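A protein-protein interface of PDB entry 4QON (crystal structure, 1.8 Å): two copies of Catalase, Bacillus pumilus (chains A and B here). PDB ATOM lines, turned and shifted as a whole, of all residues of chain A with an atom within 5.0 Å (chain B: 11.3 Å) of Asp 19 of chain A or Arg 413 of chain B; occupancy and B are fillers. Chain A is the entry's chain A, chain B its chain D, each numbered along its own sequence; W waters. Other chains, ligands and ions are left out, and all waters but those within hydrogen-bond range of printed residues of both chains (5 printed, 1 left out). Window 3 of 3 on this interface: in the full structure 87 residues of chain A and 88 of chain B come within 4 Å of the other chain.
The side-chain amino group (NZ) of Lys 142 of chain B lies within hydrogen-bond range of the backbone carbonyl oxygen (O) of Asn 20 of chain A (3.0 Å). The side-chain amide oxygen (OE1) of Gln 21 of chain A sits at hydrogen-bond distance from the side-chain amino group (NZ) of Lys 142 of chain B (2.7 Å). The guanidinium group of Arg 413 of chain B sits at hydrogen-bond distance from the backbone carbonyl oxygen of Asn 22 of chain A (3.0 Å). N of Lys 415 of chain B lies within hydrogen-bond range of OD1 of Asn 22 of chain A (3.4 Å). The side-chain hydroxyl of Ser 23 of chain A sits at hydrogen-bond distance from the side-chain carboxylate of Asp 139 of chain B, 2.6 Å away. The guanidinium group of Arg 413 of chain B is in salt-bridge range of the side-chain carboxylate of Asp 36 of chain A (2.7 Å).
OD1 of Asp 19 of chain A is in hydrogen-bond range of N of Gln 21 of chain A, at 2.9 Å. OD2 of Asp 19 of chain A sits at hydrogen-bond distance from ND2 of Asn 22 of chain A (2.9 Å). NE2 of His 38 of chain A sits at hydrogen-bond distance from OD1 of Asn 20 of chain A, at 2.9 Å. The side-chain carboxylate (OD1) of Asp 139 of chain B lies within hydrogen-bond range of the backbone NH (N) of Leu 141 of chain B. NZ of Lys 142 of chain B lies within salt-bridge range of OD2 of Asp 145 of chain B. The side-chain amino group of Lys 331 of chain B lies within hydrogen-bond range of the backbone carbonyl oxygen of Gln 414 of chain B, at 2.7 Å.
Leu 141 of chain B touches Asp 19 of chain A. Asp 19 of chain A touches Arg 413 of chain B (OD2 to CB, 3.4 Å). Asn 20 of chain A touches Asp 145 of chain B. C of Gln 21 of chain A touches CD2 of Leu 141 of chain B (3.5 Å). CA of Asn 22 of chain A touches OD2 of Asp 139 of chain B, 3.4 Å away. Asn 22 of chain A touches Leu 141 of chain B (N to CD2, 3.5 Å). CB of Asn 22 of chain A touches N of Gln 414 of chain B, 3.7 Å away. CB of Leu 141 of chain B touches OG of Ser 23 of chain A (3.9 Å). Ser 23 of chain A touches Val 412 of chain B. Arg 413 of chain B touches Ser 23 of chain A (CA to O, 3.8 Å).
No residue of chain B comes within 4 Å of Val 17 of chain A. No residue of chain B comes within 4 Å of Gly 18 of chain A. Asp 19 of chain A touches two residues of chain B. Of chain B, only Leu 141 (3.4 Å), Lys 142 (3.0 Å) and Asp 145 (3.9 Å) come within 4 Å of Asn 20 of chain A. Of the printed residues of chain B, Gln 21 of chain A touches Asp 139 (3.6 Å), Leu 141 (3.5 Å) and Lys 142 (2.7 Å). Asn 22 of chain A touches five residues of chain B. Printed residues of chain B within 4 Å of Ser 23 of chain A: Asp 139, Leu 141, Val 412 and Arg 413. Of chain B, only Met 411 (3.9 Å), Val 412 (3.3 Å) and Arg 413 (3.7 Å) come within 4 Å of Arg 24 of chain A. Asp 36 of chain A touches one residue of chain B. His 38 of chain A touches just one residue of chain B: Leu 141 (3.9 Å). Phe 143 of chain B touches none of the printed residues of chain A. Of the printed residues of chain A, Asp 145 of chain B touches Asn 20. Of the printed residues of chain A, Met 411 of chain B touches Arg 24. Of the printed residues of chain A, Val 412 of chain B touches Ser 23 (3.6 Å) and Arg 24 (3.3 Å). Arg 413 of chain B touches five residues of chain A. Printed residues of chain A within 4 Å of Gln 414 of chain B: Asn 22. Printed residues of chain A within 4 Å of Lys 415 of chain B: Asn 22.
Of the 11 printed residues of chain A, 8 touch a printed residue of chain B. Hydrophobic or aromatic side chains of chain A within 4 Å of the printed part of chain B: His 38. Of the 20 printed residues of chain B, 9 touch a printed residue of chain A. Printed residues of chain B that touch a printed residue of chain A: Asp 139, Leu 141, Lys 142, Asp 145, Met 411, Val 412, Arg 413, Gln 414 and Lys 415. Hydrophobic or aromatic side chains of chain B within 4 Å of the printed part of chain A: Leu 141 and Met 411.
No position is printed for both chains.
Water W2 lies within hydrogen-bond range of O of Ser 23 of chain A, NZ of Lys 331 of chain B, N of Gln 414 of chain B and O of Val 412 of chain B. Water W3 bridges OD1 of Asp 145 of chain B (2.6 Å) and ND2 of Asn 20 of chain A (2.9 Å). Water W5 lies within hydrogen-bond range of O of Met 411 of chain B (2.7 Å) and NE of Arg 24 of chain A (2.9 Å). Water W4 lies within hydrogen-bond range of the side-chain amide oxygen (OD1) of Asn 22 of chain A (2.7 Å), the side-chain carboxylate (OD2) of Asp 139 of chain B (2.8 Å) and the side-chain amino group (NZ) of Lys 331 of chain B (3.1 Å). Water W1 bridges O of Lys 331 of chain B (3.0 Å) and OG of Ser 23 of chain A (3.2 Å).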
ATOM      1  N   VAL A  17     -10.059  21.987  -8.759  1.00  0.00           N
ATOM      2  CA  VAL A  17      -9.625  22.537 -10.033  1.00  0.00           C
ATOM      3  C   VAL A  17      -9.550  21.422 -11.115  1.00  0.00           C
ATOM      4  O   VAL A  17      -8.828  20.423 -10.952  1.00  0.00           O
ATOM      5  CB  VAL A  17      -8.262  23.267  -9.868  1.00  0.00           C
ATOM      6  CG1 VAL A  17      -7.678  23.711 -11.201  1.00  0.00           C
ATOM      7  CG2 VAL A  17      -8.410  24.500  -9.011  1.00  0.00           C
ATOM      8  N   GLY A  18     -10.240  21.658 -12.231  1.00  0.00           N
ATOM      9  CA  GLY A  18     -10.345  20.732 -13.321  1.00  0.00           C
ATOM     10  C   GLY A  18      -9.129  20.741 -14.215  1.00  0.00           C
ATOM     11  O   GLY A  18      -8.715  19.666 -14.764  1.00  0.00           O
ATOM     12  N   ASP A  19      -8.502  21.873 -14.318  1.00  0.00           N
ATOM     13  CA  ASP A  19      -7.413  22.064 -15.228  1.00  0.00           C
ATOM     14  C   ASP A  19      -6.520  23.186 -14.696  1.00  0.00           C
ATOM     15  O   ASP A  19      -6.940  24.359 -14.661  1.00  0.00           O
ATOM     16  CB  ASP A  19      -7.973  22.387 -16.595  1.00  0.00           C
ATOM     17  CG  ASP A  19      -6.876  22.462 -17.714  1.00  0.00           C
ATOM     18  OD1 ASP A  19      -5.683  22.529 -17.361  1.00  0.00           O
ATOM     19  OD2 ASP A  19      -7.262  22.412 -18.935  1.00  0.00           O
ATOM     20  N   ASN A  20      -5.316  22.824 -14.241  1.00  0.00           N
ATOM     21  CA  ASN A  20      -4.366  23.802 -13.721  1.00  0.00           C
ATOM     22  C   ASN A  20      -3.315  24.175 -14.735  1.00  0.00           C
ATOM     23  O   ASN A  20      -2.327  24.833 -14.375  1.00  0.00           O
ATOM     24  CB  ASN A  20      -3.696  23.270 -12.460  1.00  0.00           C
ATOM     25  CG  ASN A  20      -2.942  24.344 -11.663  1.00  0.00           C
ATOM     26  OD1 ASN A  20      -3.404  25.474 -11.453  1.00  0.00           O
ATOM     27  ND2 ASN A  20      -1.770  23.969 -11.176  1.00  0.00           N
ATOM     28  N   GLN A  21      -3.523  23.803 -15.992  1.00  0.00           N
ATOM     29  CA  GLN A  21      -2.584  24.143 -17.070  1.00  0.00           C
ATOM     30  C   GLN A  21      -3.053  25.184 -18.045  1.00  0.00           C
ATOM     31  O   GLN A  21      -2.242  25.976 -18.556  1.00  0.00           O
ATOM     32  CB  GLN A  21      -2.218  22.893 -17.868  1.00  0.00           C
ATOM     33  CG  GLN A  21      -2.013  21.645 -17.051  1.00  0.00           C
ATOM     34  CD  GLN A  21      -1.152  21.840 -15.817  1.00  0.00           C
ATOM     35  OE1 GLN A  21      -0.055  22.411 -15.864  1.00  0.00           O
ATOM     36  NE2 GLN A  21      -1.618  21.254 -14.704  1.00  0.00           N
ATOM     37  N   ASN A  22      -4.328  25.146 -18.405  1.00  0.00           N
ATOM     38  CA  ASN A  22      -4.809  25.967 -19.522  1.00  0.00           C
ATOM     39  C   ASN A  22      -5.845  27.030 -19.035  1.00  0.00           C
ATOM     40  O   ASN A  22      -6.824  26.668 -18.352  1.00  0.00           O
ATOM     41  CB  ASN A  22      -5.479  25.077 -20.579  1.00  0.00           C
ATOM     42  CG  ASN A  22      -4.591  23.972 -21.064  1.00  0.00           C
ATOM     43  OD1 ASN A  22      -3.577  24.213 -21.736  1.00  0.00           O
ATOM     44  ND2 ASN A  22      -4.942  22.756 -20.700  1.00  0.00           N
ATOM     45  N   SER A  23      -5.612  28.275 -19.456  1.00  0.00           N
ATOM     46  CA  SER A  23      -6.608  29.329 -19.383  1.00  0.00           C
ATOM     47  C   SER A  23      -7.850  28.997 -20.201  1.00  0.00           C
ATOM     48  O   SER A  23      -7.778  28.261 -21.165  1.00  0.00           O
ATOM     49  CB  SER A  23      -5.977  30.624 -19.848  1.00  0.00           C
ATOM     50  OG  SER A  23      -5.000  30.977 -18.877  1.00  0.00           O
ATOM     51  N   ARG A  24      -8.991  29.644 -19.866  1.00  0.00           N
ATOM     52  CA  ARG A  24     -10.167  29.543 -20.670  1.00  0.00           C
ATOM     53  C   ARG A  24     -10.252  30.541 -21.828  1.00  0.00           C
ATOM     54  O   ARG A  24     -10.108  31.758 -21.626  1.00  0.00           O
ATOM     55  CB  ARG A  24     -11.378  29.812 -19.772  1.00  0.00           C
ATOM     56  CG  ARG A  24     -12.547  28.980 -20.124  1.00  0.00           C
ATOM     57  CD  ARG A  24     -13.613  29.223 -19.090  1.00  0.00           C
ATOM     58  NE  ARG A  24     -14.753  28.375 -19.333  1.00  0.00           N
ATOM     59  CZ  ARG A  24     -15.968  28.637 -18.884  1.00  0.00           C
ATOM     60  NH1 ARG A  24     -16.176  29.715 -18.139  1.00  0.00           N
ATOM     61  NH2 ARG A  24     -16.945  27.772 -19.141  1.00  0.00           N
ATOM     62  N   ASP A  36     -13.001  33.198 -15.776  1.00  0.00           N
ATOM     63  CA  ASP A  36     -12.013  32.117 -15.474  1.00  0.00           C
ATOM     64  C   ASP A  36     -11.590  32.405 -14.038  1.00  0.00           C
ATOM     65  O   ASP A  36     -10.584  33.081 -13.771  1.00  0.00           O
ATOM     66  CB  ASP A  36     -10.824  32.196 -16.401  1.00  0.00           C
ATOM     67  CG  ASP A  36      -9.860  30.980 -16.233  1.00  0.00           C
ATOM     68  OD1 ASP A  36      -9.951  30.285 -15.197  1.00  0.00           O
ATOM     69  OD2 ASP A  36      -9.116  30.697 -17.200  1.00  0.00           O
ATOM     70  N   TYR A  37     -12.406  31.954 -13.084  1.00  0.00           N
ATOM     71  CA  TYR A  37     -12.238  32.340 -11.717  1.00  0.00           C
ATOM     72  C   TYR A  37     -10.880  31.788 -11.211  1.00  0.00           C
ATOM     73  O   TYR A  37     -10.161  32.446 -10.488  1.00  0.00           O
ATOM     74  CB  TYR A  37     -13.406  31.788 -10.815  1.00  0.00           C
ATOM     75  CG  TYR A  37     -13.151  32.063  -9.297  1.00  0.00           C
ATOM     76  CD1 TYR A  37     -13.534  33.240  -8.738  1.00  0.00           C
ATOM     77  CD2 TYR A  37     -12.459  31.180  -8.484  1.00  0.00           C
ATOM     78  CE1 TYR A  37     -13.319  33.543  -7.442  1.00  0.00           C
ATOM     79  CE2 TYR A  37     -12.260  31.452  -7.108  1.00  0.00           C
ATOM     80  CZ  TYR A  37     -12.668  32.663  -6.602  1.00  0.00           C
ATOM     81  OH  TYR A  37     -12.465  33.013  -5.318  1.00  0.00           O
ATOM     82  N   HIS A  38     -10.538  30.580 -11.627  1.00  0.00           N
ATOM     83  CA  HIS A  38      -9.278  30.012 -11.108  1.00  0.00           C
ATOM     84  C   HIS A  38      -8.029  30.826 -11.538  1.00  0.00           C
ATOM     85  O   HIS A  38      -7.113  31.026 -10.706  1.00  0.00           O
ATOM     86  CB  HIS A  38      -9.160  28.573 -11.544  1.00  0.00           C
ATOM     87  CG  HIS A  38      -7.824  27.930 -11.197  1.00  0.00           C
ATOM     88  ND1 HIS A  38      -7.243  27.995  -9.943  1.00  0.00           N
ATOM     89  CD2 HIS A  38      -7.036  27.080 -11.915  1.00  0.00           C
ATOM     90  CE1 HIS A  38      -6.148  27.248  -9.916  1.00  0.00           C
ATOM     91  NE2 HIS A  38      -5.955  26.765 -11.122  1.00  0.00           N
ATOM     92  N   ARG B 138       3.736  29.112 -22.111  1.00  0.00           N
ATOM     93  CA  ARG B 138       2.840  29.724 -23.121  1.00  0.00           C
ATOM     94  C   ARG B 138       1.461  30.032 -22.636  1.00  0.00           C
ATOM     95  O   ARG B 138       0.621  30.425 -23.437  1.00  0.00           O
ATOM     96  CB  ARG B 138       2.745  28.834 -24.350  1.00  0.00           C
ATOM     97  CG  ARG B 138       2.194  27.435 -24.050  1.00  0.00           C
ATOM     98  CD  ARG B 138       1.843  26.652 -25.338  1.00  0.00           C
ATOM     99  NE  ARG B 138       2.998  26.343 -26.175  1.00  0.00           N
ATOM    100  CZ  ARG B 138       3.623  25.160 -26.233  1.00  0.00           C
ATOM    101  NH1 ARG B 138       3.213  24.103 -25.526  1.00  0.00           N
ATOM    102  NH2 ARG B 138       4.625  25.006 -27.046  1.00  0.00           N
ATOM    103  N   ASP B 139       1.188  29.834 -21.346  1.00  0.00           N
ATOM    104  CA  ASP B 139      -0.079  30.149 -20.771  1.00  0.00           C
ATOM    105  C   ASP B 139       0.119  30.776 -19.376  1.00  0.00           C
ATOM    106  O   ASP B 139       0.788  30.252 -18.530  1.00  0.00           O
ATOM    107  CB  ASP B 139      -0.930  28.872 -20.691  1.00  0.00           C
ATOM    108  CG  ASP B 139      -2.376  29.155 -20.314  1.00  0.00           C
ATOM    109  OD1 ASP B 139      -2.626  29.927 -19.335  1.00  0.00           O
ATOM    110  OD2 ASP B 139      -3.281  28.628 -21.030  1.00  0.00           O
ATOM    111  N   ALA B 140      -0.549  31.899 -19.126  1.00  0.00           N
ATOM    112  CA  ALA B 140      -0.335  32.602 -17.862  1.00  0.00           C
ATOM    113  C   ALA B 140      -0.794  31.893 -16.621  1.00  0.00           C
ATOM    114  O   ALA B 140      -0.288  32.188 -15.518  1.00  0.00           O
ATOM    115  CB  ALA B 140      -1.012  33.950 -17.944  1.00  0.00           C
ATOM    116  N   LEU B 141      -1.719  30.928 -16.772  1.00  0.00           N
ATOM    117  CA  LEU B 141      -2.100  30.097 -15.649  1.00  0.00           C
ATOM    118  C   LEU B 141      -0.870  29.450 -14.950  1.00  0.00           C
ATOM    119  O   LEU B 141      -0.903  29.179 -13.769  1.00  0.00           O
ATOM    120  CB  LEU B 141      -3.076  29.036 -16.105  1.00  0.00           C
ATOM    121  CG  LEU B 141      -3.756  28.184 -15.001  1.00  0.00           C
ATOM    122  CD1 LEU B 141      -4.511  29.120 -14.070  1.00  0.00           C
ATOM    123  CD2 LEU B 141      -4.689  27.186 -15.635  1.00  0.00           C
ATOM    124  N   LYS B 142       0.229  29.267 -15.693  1.00  0.00           N
ATOM    125  CA  LYS B 142       1.402  28.538 -15.114  1.00  0.00           C
ATOM    126  C   LYS B 142       2.384  29.473 -14.436  1.00  0.00           C
ATOM    127  O   LYS B 142       3.357  29.041 -13.863  1.00  0.00           O
ATOM    128  CB  LYS B 142       2.102  27.737 -16.180  1.00  0.00           C
ATOM    129  CG  LYS B 142       1.285  26.642 -16.877  1.00  0.00           C
ATOM    130  CD  LYS B 142       0.512  25.801 -15.892  1.00  0.00           C
ATOM    131  CE  LYS B 142       1.392  25.137 -14.820  1.00  0.00           C
ATOM    132  NZ  LYS B 142       0.560  24.246 -13.967  1.00  0.00           N
ATOM    133  N   PHE B 143       2.215  30.769 -14.595  1.00  0.00           N
ATOM    134  CA  PHE B 143       3.247  31.714 -14.237  1.00  0.00           C
ATOM    135  C   PHE B 143       3.523  31.690 -12.728  1.00  0.00           C
ATOM    136  O   PHE B 143       4.674  31.658 -12.378  1.00  0.00           O
ATOM    137  CB  PHE B 143       2.874  33.128 -14.689  1.00  0.00           C
ATOM    138  CG  PHE B 143       3.943  34.133 -14.482  1.00  0.00           C
ATOM    139  CD1 PHE B 143       5.103  34.099 -15.275  1.00  0.00           C
ATOM    140  CD2 PHE B 143       3.846  35.078 -13.458  1.00  0.00           C
ATOM    141  CE1 PHE B 143       6.077  35.031 -15.124  1.00  0.00           C
ATOM    142  CE2 PHE B 143       4.847  36.013 -13.309  1.00  0.00           C
ATOM    143  CZ  PHE B 143       5.969  35.966 -14.082  1.00  0.00           C
ATOM    144  N   PRO B 144       2.492  31.562 -11.847  1.00  0.00           N
ATOM    145  CA  PRO B 144       2.863  31.480 -10.421  1.00  0.00           C
ATOM    146  C   PRO B 144       3.598  30.199 -10.047  1.00  0.00           C
ATOM    147  O   PRO B 144       4.523  30.224  -9.181  1.00  0.00           O
ATOM    148  CB  PRO B 144       1.534  31.579  -9.711  1.00  0.00           C
ATOM    149  CG  PRO B 144       0.658  32.367 -10.642  1.00  0.00           C
ATOM    150  CD  PRO B 144       1.039  31.854 -12.003  1.00  0.00           C
ATOM    151  N   ASP B 145       3.261  29.115 -10.730  1.00  0.00           N
ATOM    152  CA  ASP B 145       4.030  27.859 -10.579  1.00  0.00           C
ATOM    153  C   ASP B 145       5.487  27.970 -10.972  1.00  0.00           C
ATOM    154  O   ASP B 145       6.397  27.592 -10.207  1.00  0.00           O
ATOM    155  CB  ASP B 145       3.337  26.774 -11.386  1.00  0.00           C
ATOM    156  CG  ASP B 145       1.958  26.466 -10.854  1.00  0.00           C
ATOM    157  OD1 ASP B 145       1.816  26.056  -9.691  1.00  0.00           O
ATOM    158  OD2 ASP B 145       0.994  26.618 -11.663  1.00  0.00           O
ATOM    159  N   GLU B 173       7.705  22.574 -23.050  1.00  0.00           N
ATOM    160  CA  GLU B 173       7.689  23.835 -23.826  1.00  0.00           C
ATOM    161  C   GLU B 173       8.769  24.815 -23.399  1.00  0.00           C
ATOM    162  O   GLU B 173       9.129  25.695 -24.199  1.00  0.00           O
ATOM    163  CB  GLU B 173       6.339  24.513 -23.784  1.00  0.00           C
ATOM    164  CG  GLU B 173       5.908  24.921 -22.397  1.00  0.00           C
ATOM    165  CD  GLU B 173       4.981  23.905 -21.784  1.00  0.00           C
ATOM    166  OE1 GLU B 173       5.310  22.676 -21.738  1.00  0.00           O
ATOM    167  OE2 GLU B 173       3.906  24.340 -21.377  1.00  0.00           O
ATOM    168  N   LYS B 331      -1.631  33.396 -25.205  1.00  0.00           N
ATOM    169  CA  LYS B 331      -2.336  33.150 -23.945  1.00  0.00           C
ATOM    170  C   LYS B 331      -1.479  33.620 -22.742  1.00  0.00           C
ATOM    171  O   LYS B 331      -2.002  33.905 -21.683  1.00  0.00           O
ATOM    172  CB  LYS B 331      -2.651  31.676 -23.745  1.00  0.00           C
ATOM    173  CG  LYS B 331      -3.598  31.102 -24.788  1.00  0.00           C
ATOM    174  CD  LYS B 331      -3.955  29.673 -24.449  1.00  0.00           C
ATOM    175  CE  LYS B 331      -4.627  28.979 -25.637  1.00  0.00           C
ATOM    176  NZ  LYS B 331      -4.885  27.576 -25.269  1.00  0.00           N
ATOM    177  N   GLY B 408     -12.546  29.844 -32.856  1.00  0.00           N
ATOM    178  CA  GLY B 408     -13.098  28.818 -31.974  1.00  0.00           C
ATOM    179  C   GLY B 408     -14.593  28.979 -31.781  1.00  0.00           C
ATOM    180  O   GLY B 408     -15.131  30.084 -31.790  1.00  0.00           O
ATOM    181  N   ASP B 409     -15.279  27.871 -31.603  1.00  0.00           N
ATOM    182  CA  ASP B 409     -16.728  27.920 -31.493  1.00  0.00           C
ATOM    183  C   ASP B 409     -17.217  27.688 -30.065  1.00  0.00           C
ATOM    184  O   ASP B 409     -18.399  27.857 -29.808  1.00  0.00           O
ATOM    185  CB  ASP B 409     -17.386  26.932 -32.471  1.00  0.00           C
ATOM    186  CG  ASP B 409     -17.331  25.496 -31.991  1.00  0.00           C
ATOM    187  OD1 ASP B 409     -16.352  25.104 -31.294  1.00  0.00           O
ATOM    188  OD2 ASP B 409     -18.277  24.740 -32.337  1.00  0.00           O
ATOM    189  N   ARG B 410     -16.301  27.315 -29.149  1.00  0.00           N
ATOM    190  CA  ARG B 410     -16.630  27.083 -27.722  1.00  0.00           C
ATOM    191  C   ARG B 410     -15.593  27.725 -26.784  1.00  0.00           C
ATOM    192  O   ARG B 410     -14.462  28.042 -27.190  1.00  0.00           O
ATOM    193  CB  ARG B 410     -16.672  25.598 -27.410  1.00  0.00           C
ATOM    194  CG  ARG B 410     -17.797  24.807 -28.024  1.00  0.00           C
ATOM    195  CD  ARG B 410     -17.644  23.350 -27.572  1.00  0.00           C
ATOM    196  NE  ARG B 410     -18.907  22.790 -27.049  1.00  0.00           N
ATOM    197  CZ  ARG B 410     -19.862  22.201 -27.767  1.00  0.00           C
ATOM    198  NH1 ARG B 410     -20.954  21.766 -27.155  1.00  0.00           N
ATOM    199  NH2 ARG B 410     -19.739  22.021 -29.081  1.00  0.00           N
ATOM    200  N   MET B 411     -16.023  27.902 -25.550  1.00  0.00           N
ATOM    201  CA  MET B 411     -15.163  28.310 -24.436  1.00  0.00           C
ATOM    202  C   MET B 411     -14.455  27.048 -23.968  1.00  0.00           C
ATOM    203  O   MET B 411     -15.107  26.176 -23.405  1.00  0.00           O
ATOM    204  CB  MET B 411     -16.009  28.828 -23.279  1.00  0.00           C
ATOM    205  CG  MET B 411     -16.935  30.019 -23.592  1.00  0.00           C
ATOM    206  SD  MET B 411     -17.785  30.599 -22.092  1.00  0.00           S
ATOM    207  CE  MET B 411     -16.629  31.781 -21.381  1.00  0.00           C
ATOM    208  N   VAL B 412     -13.166  26.989 -24.143  1.00  0.00           N
ATOM    209  CA  VAL B 412     -12.422  25.772 -23.869  1.00  0.00           C
ATOM    210  C   VAL B 412     -11.231  26.037 -22.942  1.00  0.00           C
ATOM    211  O   VAL B 412     -10.675  27.128 -22.912  1.00  0.00           O
ATOM    212  CB  VAL B 412     -11.986  25.059 -25.185  1.00  0.00           C
ATOM    213  CG1 VAL B 412     -13.193  24.781 -26.053  1.00  0.00           C
ATOM    214  CG2 VAL B 412     -10.892  25.831 -25.942  1.00  0.00           C
ATOM    215  N   ARG B 413     -10.777  24.996 -22.265  1.00  0.00           N
ATOM    216  CA  ARG B 413      -9.443  24.921 -21.737  1.00  0.00           C
ATOM    217  C   ARG B 413      -8.663  23.821 -22.444  1.00  0.00           C
ATOM    218  O   ARG B 413      -8.883  22.643 -22.198  1.00  0.00           O
ATOM    219  CB  ARG B 413      -9.490  24.640 -20.229  1.00  0.00           C
ATOM    220  CG  ARG B 413     -10.128  25.745 -19.395  1.00  0.00           C
ATOM    221  CD  ARG B 413     -10.000  25.341 -17.939  1.00  0.00           C
ATOM    222  NE  ARG B 413     -10.720  26.162 -16.986  1.00  0.00           N
ATOM    223  CZ  ARG B 413     -10.263  27.263 -16.411  1.00  0.00           C
ATOM    224  NH1 ARG B 413     -11.044  27.874 -15.525  1.00  0.00           N
ATOM    225  NH2 ARG B 413      -9.026  27.743 -16.672  1.00  0.00           N
ATOM    226  N   GLN B 414      -7.741  24.213 -23.323  1.00  0.00           N
ATOM    227  CA  GLN B 414      -7.066  23.270 -24.217  1.00  0.00           C
ATOM    228  C   GLN B 414      -5.774  23.852 -24.733  1.00  0.00           C
ATOM    229  O   GLN B 414      -5.765  24.980 -25.172  1.00  0.00           O
ATOM    230  CB  GLN B 414      -8.020  22.994 -25.387  1.00  0.00           C
ATOM    231  CG  GLN B 414      -7.687  21.864 -26.329  1.00  0.00           C
ATOM    232  CD  GLN B 414      -8.675  21.884 -27.492  1.00  0.00           C
ATOM    233  OE1 GLN B 414      -9.849  22.256 -27.309  1.00  0.00           O
ATOM    234  NE2 GLN B 414      -8.198  21.573 -28.686  1.00  0.00           N
ATOM    235  N   LYS B 415      -4.678  23.063 -24.726  1.00  0.00           N
ATOM    236  CA  LYS B 415      -3.423  23.499 -25.313  1.00  0.00           C
ATOM    237  C   LYS B 415      -3.597  23.883 -26.803  1.00  0.00           C
ATOM    238  O   LYS B 415      -4.408  23.321 -27.513  1.00  0.00           O
ATOM    239  CB  LYS B 415      -2.356  22.381 -25.156  1.00  0.00           C
ATOM    240  CG  LYS B 415      -0.941  22.804 -25.511  1.00  0.00           C
ATOM    241  CD  LYS B 415       0.037  21.643 -25.493  1.00  0.00           C
ATOM    242  CE  LYS B 415       0.203  21.006 -24.123  1.00  0.00           C
ATOM    243  NZ  LYS B 415       1.238  19.904 -24.239  1.00  0.00           N
ATOM    244  N   ILE B 416      -2.814  24.831 -27.268  1.00  0.00           N
ATOM    245  CA  ILE B 416      -2.771  25.141 -28.696  1.00  0.00           C
ATOM    246  C   ILE B 416      -2.393  23.886 -29.444  1.00  0.00           C
ATOM    247  O   ILE B 416      -1.608  23.030 -28.944  1.00  0.00           O
ATOM    248  CB  ILE B 416      -1.732  26.272 -29.037  1.00  0.00           C
ATOM    249  CG1 ILE B 416      -0.339  25.942 -28.470  1.00  0.00           C
ATOM    250  CG2 ILE B 416      -2.147  27.635 -28.467  1.00  0.00           C
ATOM    251  CD1 ILE B 416       0.759  26.743 -29.146  1.00  0.00           C
ATOM    252  N   GLU B 417      -2.846  23.848 -30.686  1.00  0.00           N
ATOM    253  CA  GLU B 417      -2.318  22.897 -31.655  1.00  0.00           C
ATOM    254  C   GLU B 417      -0.891  23.310 -32.111  1.00  0.00           C
ATOM    255  O   GLU B 417      -0.434  24.433 -31.872  1.00  0.00           O
ATOM    256  CB  GLU B 417      -3.329  22.731 -32.813  1.00  0.00           C
ATOM    257  CG  GLU B 417      -4.581  21.957 -32.362  1.00  0.00           C
ATOM    258  CD  GLU B 417      -5.831  22.281 -33.155  1.00  0.00           C
ATOM    259  OE1 GLU B 417      -5.739  22.865 -34.262  1.00  0.00           O
ATOM    260  OE2 GLU B 417      -6.931  21.942 -32.672  1.00  0.00           O
HETATM  261  O   HOH W   1      -4.581  33.873 -20.191  1.00  0.00           O
HETATM  262  O   HOH W   2      -7.342  27.301 -23.533  1.00  0.00           O
HETATM  263  O   HOH W   3      -0.510  25.172  -8.805  1.00  0.00           O
HETATM  264  O   HOH W   4      -3.039  26.601 -22.981  1.00  0.00           O
HETATM  265  O   HOH W   5     -14.271  26.014 -20.894  1.00  0.00           O
